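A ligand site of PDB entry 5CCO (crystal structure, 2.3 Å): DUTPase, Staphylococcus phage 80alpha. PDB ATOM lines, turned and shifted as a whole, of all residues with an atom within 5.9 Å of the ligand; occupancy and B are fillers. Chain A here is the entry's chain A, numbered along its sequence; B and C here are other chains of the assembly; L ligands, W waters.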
ATOM      1  N   ARG A 160     -14.595  27.713 -16.951  1.00  0.00           N
ATOM      2  CA  ARG A 160     -15.940  27.176 -16.647  1.00  0.00           C
ATOM      3  C   ARG A 160     -17.116  27.988 -17.226  1.00  0.00           C
ATOM      4  O   ARG A 160     -18.078  27.410 -17.745  1.00  0.00           O
ATOM      5  CB  ARG A 160     -16.103  27.026 -15.109  1.00  0.00           C
ATOM      6  CG  ARG A 160     -17.496  26.603 -14.637  1.00  0.00           C
ATOM      7  CD  ARG A 160     -17.493  26.058 -13.214  1.00  0.00           C
ATOM      8  NE  ARG A 160     -17.007  24.678 -13.120  1.00  0.00           N
ATOM      9  CZ  ARG A 160     -17.719  23.580 -13.425  1.00  0.00           C
ATOM     10  NH1 ARG A 160     -18.964  23.655 -13.874  1.00  0.00           N
ATOM     11  NH2 ARG A 160     -17.166  22.376 -13.284  1.00  0.00           N
ATOM     12  N   LYS A 163     -21.289  27.137 -17.286  1.00  0.00           N
ATOM     13  CA  LYS A 163     -21.532  25.689 -17.254  1.00  0.00           C
ATOM     14  C   LYS A 163     -21.706  25.115 -15.817  1.00  0.00           C
ATOM     15  O   LYS A 163     -20.947  25.419 -14.893  1.00  0.00           O
ATOM     16  CB  LYS A 163     -20.393  24.971 -17.996  1.00  0.00           C
ATOM     17  N   GLY A 164     -22.752  24.319 -15.629  1.00  0.00           N
ATOM     18  CA  GLY A 164     -23.091  23.722 -14.348  1.00  0.00           C
ATOM     19  C   GLY A 164     -24.083  22.602 -14.566  1.00  0.00           C
ATOM     20  O   GLY A 164     -24.640  22.473 -15.676  1.00  0.00           O
ATOM     21  N   PHE A 165     -24.299  21.795 -13.508  1.00  0.00           N
ATOM     22  CA  PHE A 165     -25.189  20.623 -13.572  1.00  0.00           C
ATOM     23  C   PHE A 165     -24.941  19.747 -14.796  1.00  0.00           C
ATOM     24  O   PHE A 165     -25.897  19.282 -15.440  1.00  0.00           O
ATOM     25  CB  PHE A 165     -26.648  21.063 -13.493  1.00  0.00           C
ATOM     26  CG  PHE A 165     -27.011  21.777 -12.222  1.00  0.00           C
ATOM     27  CD1 PHE A 165     -27.399  21.049 -11.085  1.00  0.00           C
ATOM     28  CD2 PHE A 165     -26.956  23.171 -12.150  1.00  0.00           C
ATOM     29  CE1 PHE A 165     -27.743  21.707  -9.905  1.00  0.00           C
ATOM     30  CE2 PHE A 165     -27.290  23.825 -10.969  1.00  0.00           C
ATOM     31  CZ  PHE A 165     -27.701  23.085  -9.856  1.00  0.00           C
ATOM     32  N   GLY A 166     -23.663  19.540 -15.113  1.00  0.00           N
ATOM     33  CA  GLY A 166     -23.272  18.781 -16.310  1.00  0.00           C
ATOM     34  C   GLY A 166     -23.509  17.289 -16.107  1.00  0.00           C
ATOM     35  O   GLY A 166     -23.716  16.810 -14.986  1.00  0.00           O
ATOM     36  N   SER A 167     -23.465  16.557 -17.218  1.00  0.00           N
ATOM     37  CA  SER A 167     -23.592  15.094 -17.200  1.00  0.00           C
ATOM     38  C   SER A 167     -22.281  14.430 -16.702  1.00  0.00           C
ATOM     39  O   SER A 167     -21.309  15.109 -16.380  1.00  0.00           O
ATOM     40  CB  SER A 167     -24.011  14.590 -18.585  1.00  0.00           C
ATOM     41  OG  SER A 167     -22.987  14.773 -19.540  1.00  0.00           O
ATOM     42  N   ASP B  24     -11.376  24.527 -10.412  1.00  0.00           N
ATOM     43  CA  ASP B  24     -12.477  23.832  -9.682  1.00  0.00           C
ATOM     44  C   ASP B  24     -12.039  23.374  -8.318  1.00  0.00           C
ATOM     45  O   ASP B  24     -10.855  23.153  -8.063  1.00  0.00           O
ATOM     46  CB  ASP B  24     -12.996  22.595 -10.449  1.00  0.00           C
ATOM     47  CG  ASP B  24     -14.025  22.944 -11.509  1.00  0.00           C
ATOM     48  OD1 ASP B  24     -14.352  24.128 -11.701  1.00  0.00           O
ATOM     49  OD2 ASP B  24     -14.506  22.013 -12.175  1.00  0.00           O
ATOM     50  N   ARG B  64     -21.893  15.099  -6.819  1.00  0.00           N
ATOM     51  CA  ARG B  64     -21.827  15.959  -7.994  1.00  0.00           C
ATOM     52  C   ARG B  64     -23.200  16.564  -8.266  1.00  0.00           C
ATOM     53  O   ARG B  64     -24.222  15.928  -7.995  1.00  0.00           O
ATOM     54  CB  ARG B  64     -21.348  15.149  -9.196  1.00  0.00           C
ATOM     55  CG  ARG B  64     -19.898  14.721  -9.054  1.00  0.00           C
ATOM     56  CD  ARG B  64     -19.410  13.866 -10.220  1.00  0.00           C
ATOM     57  NE  ARG B  64     -19.696  14.531 -11.491  1.00  0.00           N
ATOM     58  CZ  ARG B  64     -19.052  15.593 -11.958  1.00  0.00           C
ATOM     59  NH1 ARG B  64     -19.428  16.126 -13.106  1.00  0.00           N
ATOM     60  NH2 ARG B  64     -18.017  16.124 -11.296  1.00  0.00           N
ATOM     61  N   SER B  65     -23.219  17.743  -8.876  1.00  0.00           N
ATOM     62  CA  SER B  65     -24.464  18.461  -9.102  1.00  0.00           C
ATOM     63  C   SER B  65     -25.403  17.705 -10.076  1.00  0.00           C
ATOM     64  O   SER B  65     -26.634  17.679  -9.878  1.00  0.00           O
ATOM     65  CB  SER B  65     -24.174  19.909  -9.548  1.00  0.00           C
ATOM     66  OG  SER B  65     -23.703  19.984 -10.908  1.00  0.00           O
ATOM     67  N   GLY B  66     -24.823  17.080 -11.113  1.00  0.00           N
ATOM     68  CA  GLY B  66     -25.605  16.384 -12.110  1.00  0.00           C
ATOM     69  C   GLY B  66     -26.370  15.189 -11.539  1.00  0.00           C
ATOM     70  O   GLY B  66     -27.592  15.096 -11.661  1.00  0.00           O
ATOM     71  N   ARG B 134     -18.386   8.454 -12.805  1.00  0.00           N
ATOM     72  CA  ARG B 134     -18.022   9.602 -12.044  1.00  0.00           C
ATOM     73  C   ARG B 134     -19.243   9.940 -11.183  1.00  0.00           C
ATOM     74  O   ARG B 134     -20.244  10.456 -11.695  1.00  0.00           O
ATOM     75  CB  ARG B 134     -17.744  10.666 -13.097  1.00  0.00           C
ATOM     76  CG  ARG B 134     -17.280  12.034 -12.697  1.00  0.00           C
ATOM     77  CD  ARG B 134     -17.607  12.911 -13.898  1.00  0.00           C
ATOM     78  NE  ARG B 134     -16.865  14.165 -13.951  1.00  0.00           N
ATOM     79  CZ  ARG B 134     -17.025  15.095 -14.903  1.00  0.00           C
ATOM     80  NH1 ARG B 134     -17.925  14.959 -15.884  1.00  0.00           N
ATOM     81  NH2 ARG B 134     -16.280  16.204 -14.844  1.00  0.00           N
ATOM     82  N   GLN B 137     -17.140  13.612  -5.808  1.00  0.00           N
ATOM     83  CA  GLN B 137     -15.934  14.411  -5.861  1.00  0.00           C
ATOM     84  C   GLN B 137     -15.338  14.582  -4.475  1.00  0.00           C
ATOM     85  O   GLN B 137     -16.040  14.480  -3.465  1.00  0.00           O
ATOM     86  CB  GLN B 137     -16.210  15.773  -6.514  1.00  0.00           C
ATOM     87  CG  GLN B 137     -17.281  16.589  -5.819  1.00  0.00           C
ATOM     88  CD  GLN B 137     -17.470  17.996  -6.411  1.00  0.00           C
ATOM     89  OE1 GLN B 137     -16.499  18.697  -6.658  1.00  0.00           O
ATOM     90  NE2 GLN B 137     -18.741  18.424  -6.594  1.00  0.00           N
ATOM     91  N   LEU C  61     -23.400  26.084  -1.046  1.00  0.00           N
ATOM     92  CA  LEU C  61     -24.770  26.578  -1.170  1.00  0.00           C
ATOM     93  C   LEU C  61     -25.683  25.564  -0.464  1.00  0.00           C
ATOM     94  O   LEU C  61     -25.960  24.463  -0.965  1.00  0.00           O
ATOM     95  CB  LEU C  61     -25.148  26.782  -2.637  1.00  0.00           C
ATOM     96  CG  LEU C  61     -26.548  27.374  -2.905  1.00  0.00           C
ATOM     97  CD1 LEU C  61     -26.637  28.828  -2.501  1.00  0.00           C
ATOM     98  CD2 LEU C  61     -26.863  27.278  -4.384  1.00  0.00           C
ATOM     99  N   GLU C  76     -29.662  19.856  -1.199  1.00  0.00           N
ATOM    100  CA  GLU C  76     -28.327  19.262  -1.317  1.00  0.00           C
ATOM    101  C   GLU C  76     -27.311  20.395  -1.452  1.00  0.00           C
ATOM    102  O   GLU C  76     -27.425  21.235  -2.364  1.00  0.00           O
ATOM    103  CB  GLU C  76     -28.265  18.314  -2.514  1.00  0.00           C
ATOM    104  CG  GLU C  76     -26.863  17.739  -2.759  1.00  0.00           C
ATOM    105  CD  GLU C  76     -26.413  16.718  -1.730  1.00  0.00           C
ATOM    106  OE1 GLU C  76     -27.266  16.276  -0.915  1.00  0.00           O
ATOM    107  OE2 GLU C  76     -25.214  16.325  -1.747  1.00  0.00           O
ATOM    108  N   THR C  77     -26.307  20.382  -0.582  1.00  0.00           N
ATOM    109  CA  THR C  77     -25.199  21.336  -0.638  1.00  0.00           C
ATOM    110  C   THR C  77     -24.509  21.367  -1.985  1.00  0.00           C
ATOM    111  O   THR C  77     -24.046  20.342  -2.501  1.00  0.00           O
ATOM    112  CB  THR C  77     -24.203  21.117   0.506  1.00  0.00           C
ATOM    113  OG1 THR C  77     -24.889  21.453   1.710  1.00  0.00           O
ATOM    114  CG2 THR C  77     -22.946  22.058   0.425  1.00  0.00           C
ATOM    115  N   GLY C  78     -24.529  22.552  -2.574  1.00  0.00           N
ATOM    116  CA  GLY C  78     -23.906  22.752  -3.862  1.00  0.00           C
ATOM    117  C   GLY C  78     -22.520  23.235  -3.593  1.00  0.00           C
ATOM    118  O   GLY C  78     -22.338  24.122  -2.751  1.00  0.00           O
ATOM    119  N   LYS C  79     -21.557  22.655  -4.304  1.00  0.00           N
ATOM    120  CA  LYS C  79     -20.169  23.099  -4.270  1.00  0.00           C
ATOM    121  C   LYS C  79     -20.035  24.041  -5.464  1.00  0.00           C
ATOM    122  O   LYS C  79     -20.113  23.612  -6.606  1.00  0.00           O
ATOM    123  CB  LYS C  79     -19.195  21.924  -4.377  1.00  0.00           C
ATOM    124  CG  LYS C  79     -18.964  21.187  -3.071  1.00  0.00           C
ATOM    125  CD  LYS C  79     -20.236  20.527  -2.518  1.00  0.00           C
ATOM    126  CE  LYS C  79     -20.741  19.434  -3.466  1.00  0.00           C
ATOM    127  NZ  LYS C  79     -21.816  18.570  -2.892  1.00  0.00           N
ATOM    128  N   ILE C  80     -19.898  25.326  -5.169  1.00  0.00           N
ATOM    129  CA  ILE C  80     -19.867  26.364  -6.153  1.00  0.00           C
ATOM    130  C   ILE C  80     -18.397  26.687  -6.517  1.00  0.00           C
ATOM    131  O   ILE C  80     -17.647  27.255  -5.711  1.00  0.00           O
ATOM    132  CB  ILE C  80     -20.606  27.616  -5.646  1.00  0.00           C
ATOM    133  CG1 ILE C  80     -21.980  27.247  -5.050  1.00  0.00           C
ATOM    134  CG2 ILE C  80     -20.777  28.624  -6.783  1.00  0.00           C
ATOM    135  CD1 ILE C  80     -22.942  26.552  -5.991  1.00  0.00           C
ATOM    136  N   ASP C  81     -18.018  26.292  -7.731  1.00  0.00           N
ATOM    137  CA  ASP C  81     -16.622  26.360  -8.180  1.00  0.00           C
ATOM    138  C   ASP C  81     -16.169  27.808  -8.343  1.00  0.00           C
ATOM    139  O   ASP C  81     -16.973  28.685  -8.705  1.00  0.00           O
ATOM    140  CB  ASP C  81     -16.403  25.524  -9.485  1.00  0.00           C
ATOM    141  CG  ASP C  81     -16.549  23.970  -9.250  1.00  0.00           C
ATOM    142  OD1 ASP C  81     -15.643  23.351  -8.665  1.00  0.00           O
ATOM    143  OD2 ASP C  81     -17.555  23.349  -9.639  1.00  0.00           O
ATOM    144  N   TYR C  84     -17.136  29.737 -11.735  1.00  0.00           N
ATOM    145  CA  TYR C  84     -18.554  29.583 -12.160  1.00  0.00           C
ATOM    146  C   TYR C  84     -19.361  30.891 -12.088  1.00  0.00           C
ATOM    147  O   TYR C  84     -19.582  31.427 -10.980  1.00  0.00           O
ATOM    148  CB  TYR C  84     -19.311  28.565 -11.315  1.00  0.00           C
ATOM    149  CG  TYR C  84     -20.801  28.406 -11.691  1.00  0.00           C
ATOM    150  CD1 TYR C  84     -21.184  27.735 -12.846  1.00  0.00           C
ATOM    151  CD2 TYR C  84     -21.816  28.916 -10.881  1.00  0.00           C
ATOM    152  CE1 TYR C  84     -22.528  27.552 -13.170  1.00  0.00           C
ATOM    153  CE2 TYR C  84     -23.159  28.739 -11.183  1.00  0.00           C
ATOM    154  CZ  TYR C  84     -23.509  28.047 -12.327  1.00  0.00           C
ATOM    155  OH  TYR C  84     -24.841  27.890 -12.663  1.00  0.00           O
ATOM    156  N   ASN C  87     -26.072  31.143 -13.173  1.00  0.00           N
ATOM    157  CA  ASN C  87     -27.154  31.320 -12.219  1.00  0.00           C
ATOM    158  C   ASN C  87     -27.039  30.239 -11.140  1.00  0.00           C
ATOM    159  O   ASN C  87     -26.982  29.045 -11.466  1.00  0.00           O
ATOM    160  CB  ASN C  87     -28.491  31.198 -12.947  1.00  0.00           C
ATOM    161  CG  ASN C  87     -29.668  31.636 -12.115  1.00  0.00           C
ATOM    162  OD1 ASN C  87     -29.664  31.538 -10.891  1.00  0.00           O
ATOM    163  ND2 ASN C  87     -30.703  32.100 -12.803  1.00  0.00           N
ATOM    164  N   LEU C  88     -26.950  30.648  -9.876  1.00  0.00           N
ATOM    165  CA  LEU C  88     -26.919  29.720  -8.747  1.00  0.00           C
ATOM    166  C   LEU C  88     -28.256  28.999  -8.609  1.00  0.00           C
ATOM    167  O   LEU C  88     -29.307  29.640  -8.520  1.00  0.00           O
ATOM    168  CB  LEU C  88     -26.576  30.443  -7.440  1.00  0.00           C
ATOM    169  CG  LEU C  88     -25.191  31.077  -7.367  1.00  0.00           C
ATOM    170  CD1 LEU C  88     -25.083  31.882  -6.087  1.00  0.00           C
ATOM    171  CD2 LEU C  88     -24.148  29.984  -7.400  1.00  0.00           C
ATOM    172  N   GLY C  89     -28.173  27.667  -8.620  1.00  0.00           N
ATOM    173  CA  GLY C  89     -29.316  26.781  -8.575  1.00  0.00           C
ATOM    174  C   GLY C  89     -29.420  26.116  -7.223  1.00  0.00           C
ATOM    175  O   GLY C  89     -28.446  25.528  -6.736  1.00  0.00           O
ATOM    176  N   ILE C  90     -30.603  26.211  -6.618  1.00  0.00           N
ATOM    177  CA  ILE C  90     -30.918  25.537  -5.356  1.00  0.00           C
ATOM    178  C   ILE C  90     -31.495  24.156  -5.677  1.00  0.00           C
ATOM    179  O   ILE C  90     -32.596  24.032  -6.191  1.00  0.00           O
ATOM    180  CB  ILE C  90     -31.845  26.365  -4.451  1.00  0.00           C
ATOM    181  CG1 ILE C  90     -31.175  27.726  -4.162  1.00  0.00           C
ATOM    182  CG2 ILE C  90     -32.109  25.615  -3.149  1.00  0.00           C
ATOM    183  CD1 ILE C  90     -32.147  28.769  -3.701  1.00  0.00           C
ATOM    184  N   ASN C  91     -30.684  23.144  -5.388  1.00  0.00           N
ATOM    185  CA  ASN C  91     -30.957  21.762  -5.701  1.00  0.00           C
ATOM    186  C   ASN C  91     -31.744  21.155  -4.531  1.00  0.00           C
ATOM    187  O   ASN C  91     -31.194  20.892  -3.457  1.00  0.00           O
ATOM    188  CB  ASN C  91     -29.608  21.069  -5.911  1.00  0.00           C
ATOM    189  CG  ASN C  91     -29.703  19.620  -6.316  1.00  0.00           C
ATOM    190  OD1 ASN C  91     -30.738  19.121  -6.764  1.00  0.00           O
ATOM    191  ND2 ASN C  91     -28.587  18.937  -6.170  1.00  0.00           N
HETATM  192  N1  LIG L   1     -24.111  24.385  -9.076  1.00  0.00           N
HETATM  193  C1  LIG L   1     -25.190  25.126  -8.583  1.00  0.00           C
HETATM  194  N2  LIG L   1     -25.920  24.679  -7.525  1.00  0.00           N
HETATM  195  C2  LIG L   1     -25.658  23.503  -6.935  1.00  0.00           C
HETATM  196  C3  LIG L   1     -24.602  22.739  -7.403  1.00  0.00           C
HETATM  197  C4  LIG L   1     -23.818  23.210  -8.468  1.00  0.00           C
HETATM  198  O1  LIG L   1     -25.494  26.217  -9.115  1.00  0.00           O
HETATM  199  O2  LIG L   1     -26.353  23.087  -5.979  1.00  0.00           O
HETATM  200  C5  LIG L   1     -23.316  24.887 -10.210  1.00  0.00           C
HETATM  201  C6  LIG L   1     -22.069  25.666  -9.746  1.00  0.00           C
HETATM  202  C7  LIG L   1     -20.955  24.659  -9.898  1.00  0.00           C
HETATM  203  C8  LIG L   1     -21.422  23.809 -11.065  1.00  0.00           C
HETATM  204  O3  LIG L   1     -19.693  25.273 -10.154  1.00  0.00           O
HETATM  205  O4  LIG L   1     -22.860  23.792 -11.013  1.00  0.00           O
HETATM  206  C9  LIG L   1     -20.836  22.415 -11.038  1.00  0.00           C
HETATM  207  O5  LIG L   1     -21.362  21.694 -12.168  1.00  0.00           O
HETATM  208  P1  LIG L   1     -20.677  20.289 -12.571  1.00  0.00           P
HETATM  209  O6  LIG L   1     -21.091  20.093 -14.021  1.00  0.00           O
HETATM  210  O7  LIG L   1     -19.225  20.496 -12.348  1.00  0.00           O
HETATM  211  O8  LIG L   1     -21.261  19.277 -11.597  1.00  0.00           O
HETATM  212  O   HOH W   1     -26.241  20.410  -5.012  1.00  0.00           O
HETATM  213  O   HOH W   2     -20.276  21.516 -15.808  1.00  0.00           O
HETATM  214  O   HOH W   3     -17.806  20.704 -10.411  1.00  0.00           O
HETATM  215  O   HOH W   4     -28.098  23.599  -3.826  1.00  0.00           O
HETATM  216  O   HOH W   5     -22.311  17.111 -12.416  1.00  0.00           O
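The backbone NH (N) of Gly 89 of chain C lies within hydrogen-bond range of an oxygen (O1) of the ligand (3.1 Å). N of Asp 81 of chain C is in hydrogen-bond range of O3 of the ligand (3.1 Å). An oxygen (O5) of the ligand lies within hydrogen-bond range of the backbone NH (N) of Phe 165 (3.2 Å). NH1 of Arg 64 of chain B lies within salt-bridge range of O8 of the ligand (3.9 Å). O of Gly 89 of chain C lies within hydrogen-bond range of N2 of the ligand (2.8 Å). The guanidinium group of Arg 160 lies within salt-bridge range of an oxygen (O7) of the ligand, 2.9 Å away. N of Gly 166 lies within hydrogen-bond range of O6 of the ligand (2.8 Å). The side-chain hydroxyl (OG) of Ser 65 of chain B lies within hydrogen-bond range of an oxygen (O8) of the ligand (2.6 Å). The side-chain carboxylate (OD2) of Asp 81 of chain C sits at hydrogen-bond distance from an oxygen (O3) of the ligand, 2.9 Å away.
Water W3 lies within hydrogen-bond range of O7 of the ligand, OD2 of Asp 81 of chain C and NH2 of Arg 160. Water W2 bridges an oxygen (O6) of the ligand and the guanidinium group of Arg 160. Water W5 lies within hydrogen-bond range of an oxygen (O8) of the ligand (2.5 Å), the backbone NH of Gly 66 of chain B (2.8 Å), the backbone carbonyl oxygen of Gly 166 (2.9 Å) and the guanidinium group of Arg 64 of chain B (3.1 Å). Water W4 lies within hydrogen-bond range of an oxygen (O2) of the ligand (2.8 Å), the backbone carbonyl oxygen of Glu 76 of chain C (2.9 Å) and the backbone NH of Asn 91 of chain C (3.1 Å).
NH1 of Arg 160 is in hydrogen-bond range of O of Lys 163 (2.8 Å). The guanidinium group of Arg 160 is in salt-bridge range of the side-chain carboxylate of Asp 81 of chain C (3.8 Å). OD2 of Asp 24 of chain B lies within salt-bridge range of NH2 of Arg 160 (2.9 Å). The side-chain hydroxyl of Tyr 84 of chain C lies within hydrogen-bond range of the backbone carbonyl oxygen of Asn 87 of chain C (2.7 Å). O of Asn 91 of chain C lies within hydrogen-bond range of N of Glu 76 of chain C (2.9 Å). O of Gly 78 of chain C is in hydrogen-bond range of N of Leu 61 of chain C (2.8 Å). The side-chain amino group (NZ) of Lys 79 of chain C is in hydrogen-bond range of the backbone carbonyl oxygen (O) of Thr 77 of chain C. The side-chain hydroxyl (OG) of Ser 65 of chain B sits close to the backbone NH (N) of Phe 165 (3.2 Å).
Gly 164 touches the ligand. Gly 78 of chain C touches the ligand (CA to O2, 3.3 Å). Lys 79 of chain C touches the ligand (O to C7, 3.6 Å). Ile 80 of chain C touches the ligand (CD1 to C1, 3.7 Å). Tyr 84 of chain C touches the ligand (CD2 to C6, 3.5 Å). O of Asn 87 of chain C touches O1 of the ligand, 3.97 Å away. CA of Leu 88 of chain C touches O1 of the ligand, 3.8 Å away. Asn 91 of chain C touches the ligand (CB to O2, 3.8 Å). Hydrophobic or aromatic side chains that line the ligand: Phe 165, Ile 80 of chain C and Tyr 84 of chain C. 15 residues have an atom within 4 Å of the ligand: Arg 160, Gly 164, Phe 165, Gly 166, Arg 64 of chain B, Ser 65 of chain B, Gly 78 of chain C, Lys 79 of chain C, Ile 80 of chain C, Asp 81 of chain C, Tyr 84 of chain C, Asn 87 of chain C, Leu 88 of chain C, Gly 89 of chain C and Asn 91 of chain C.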
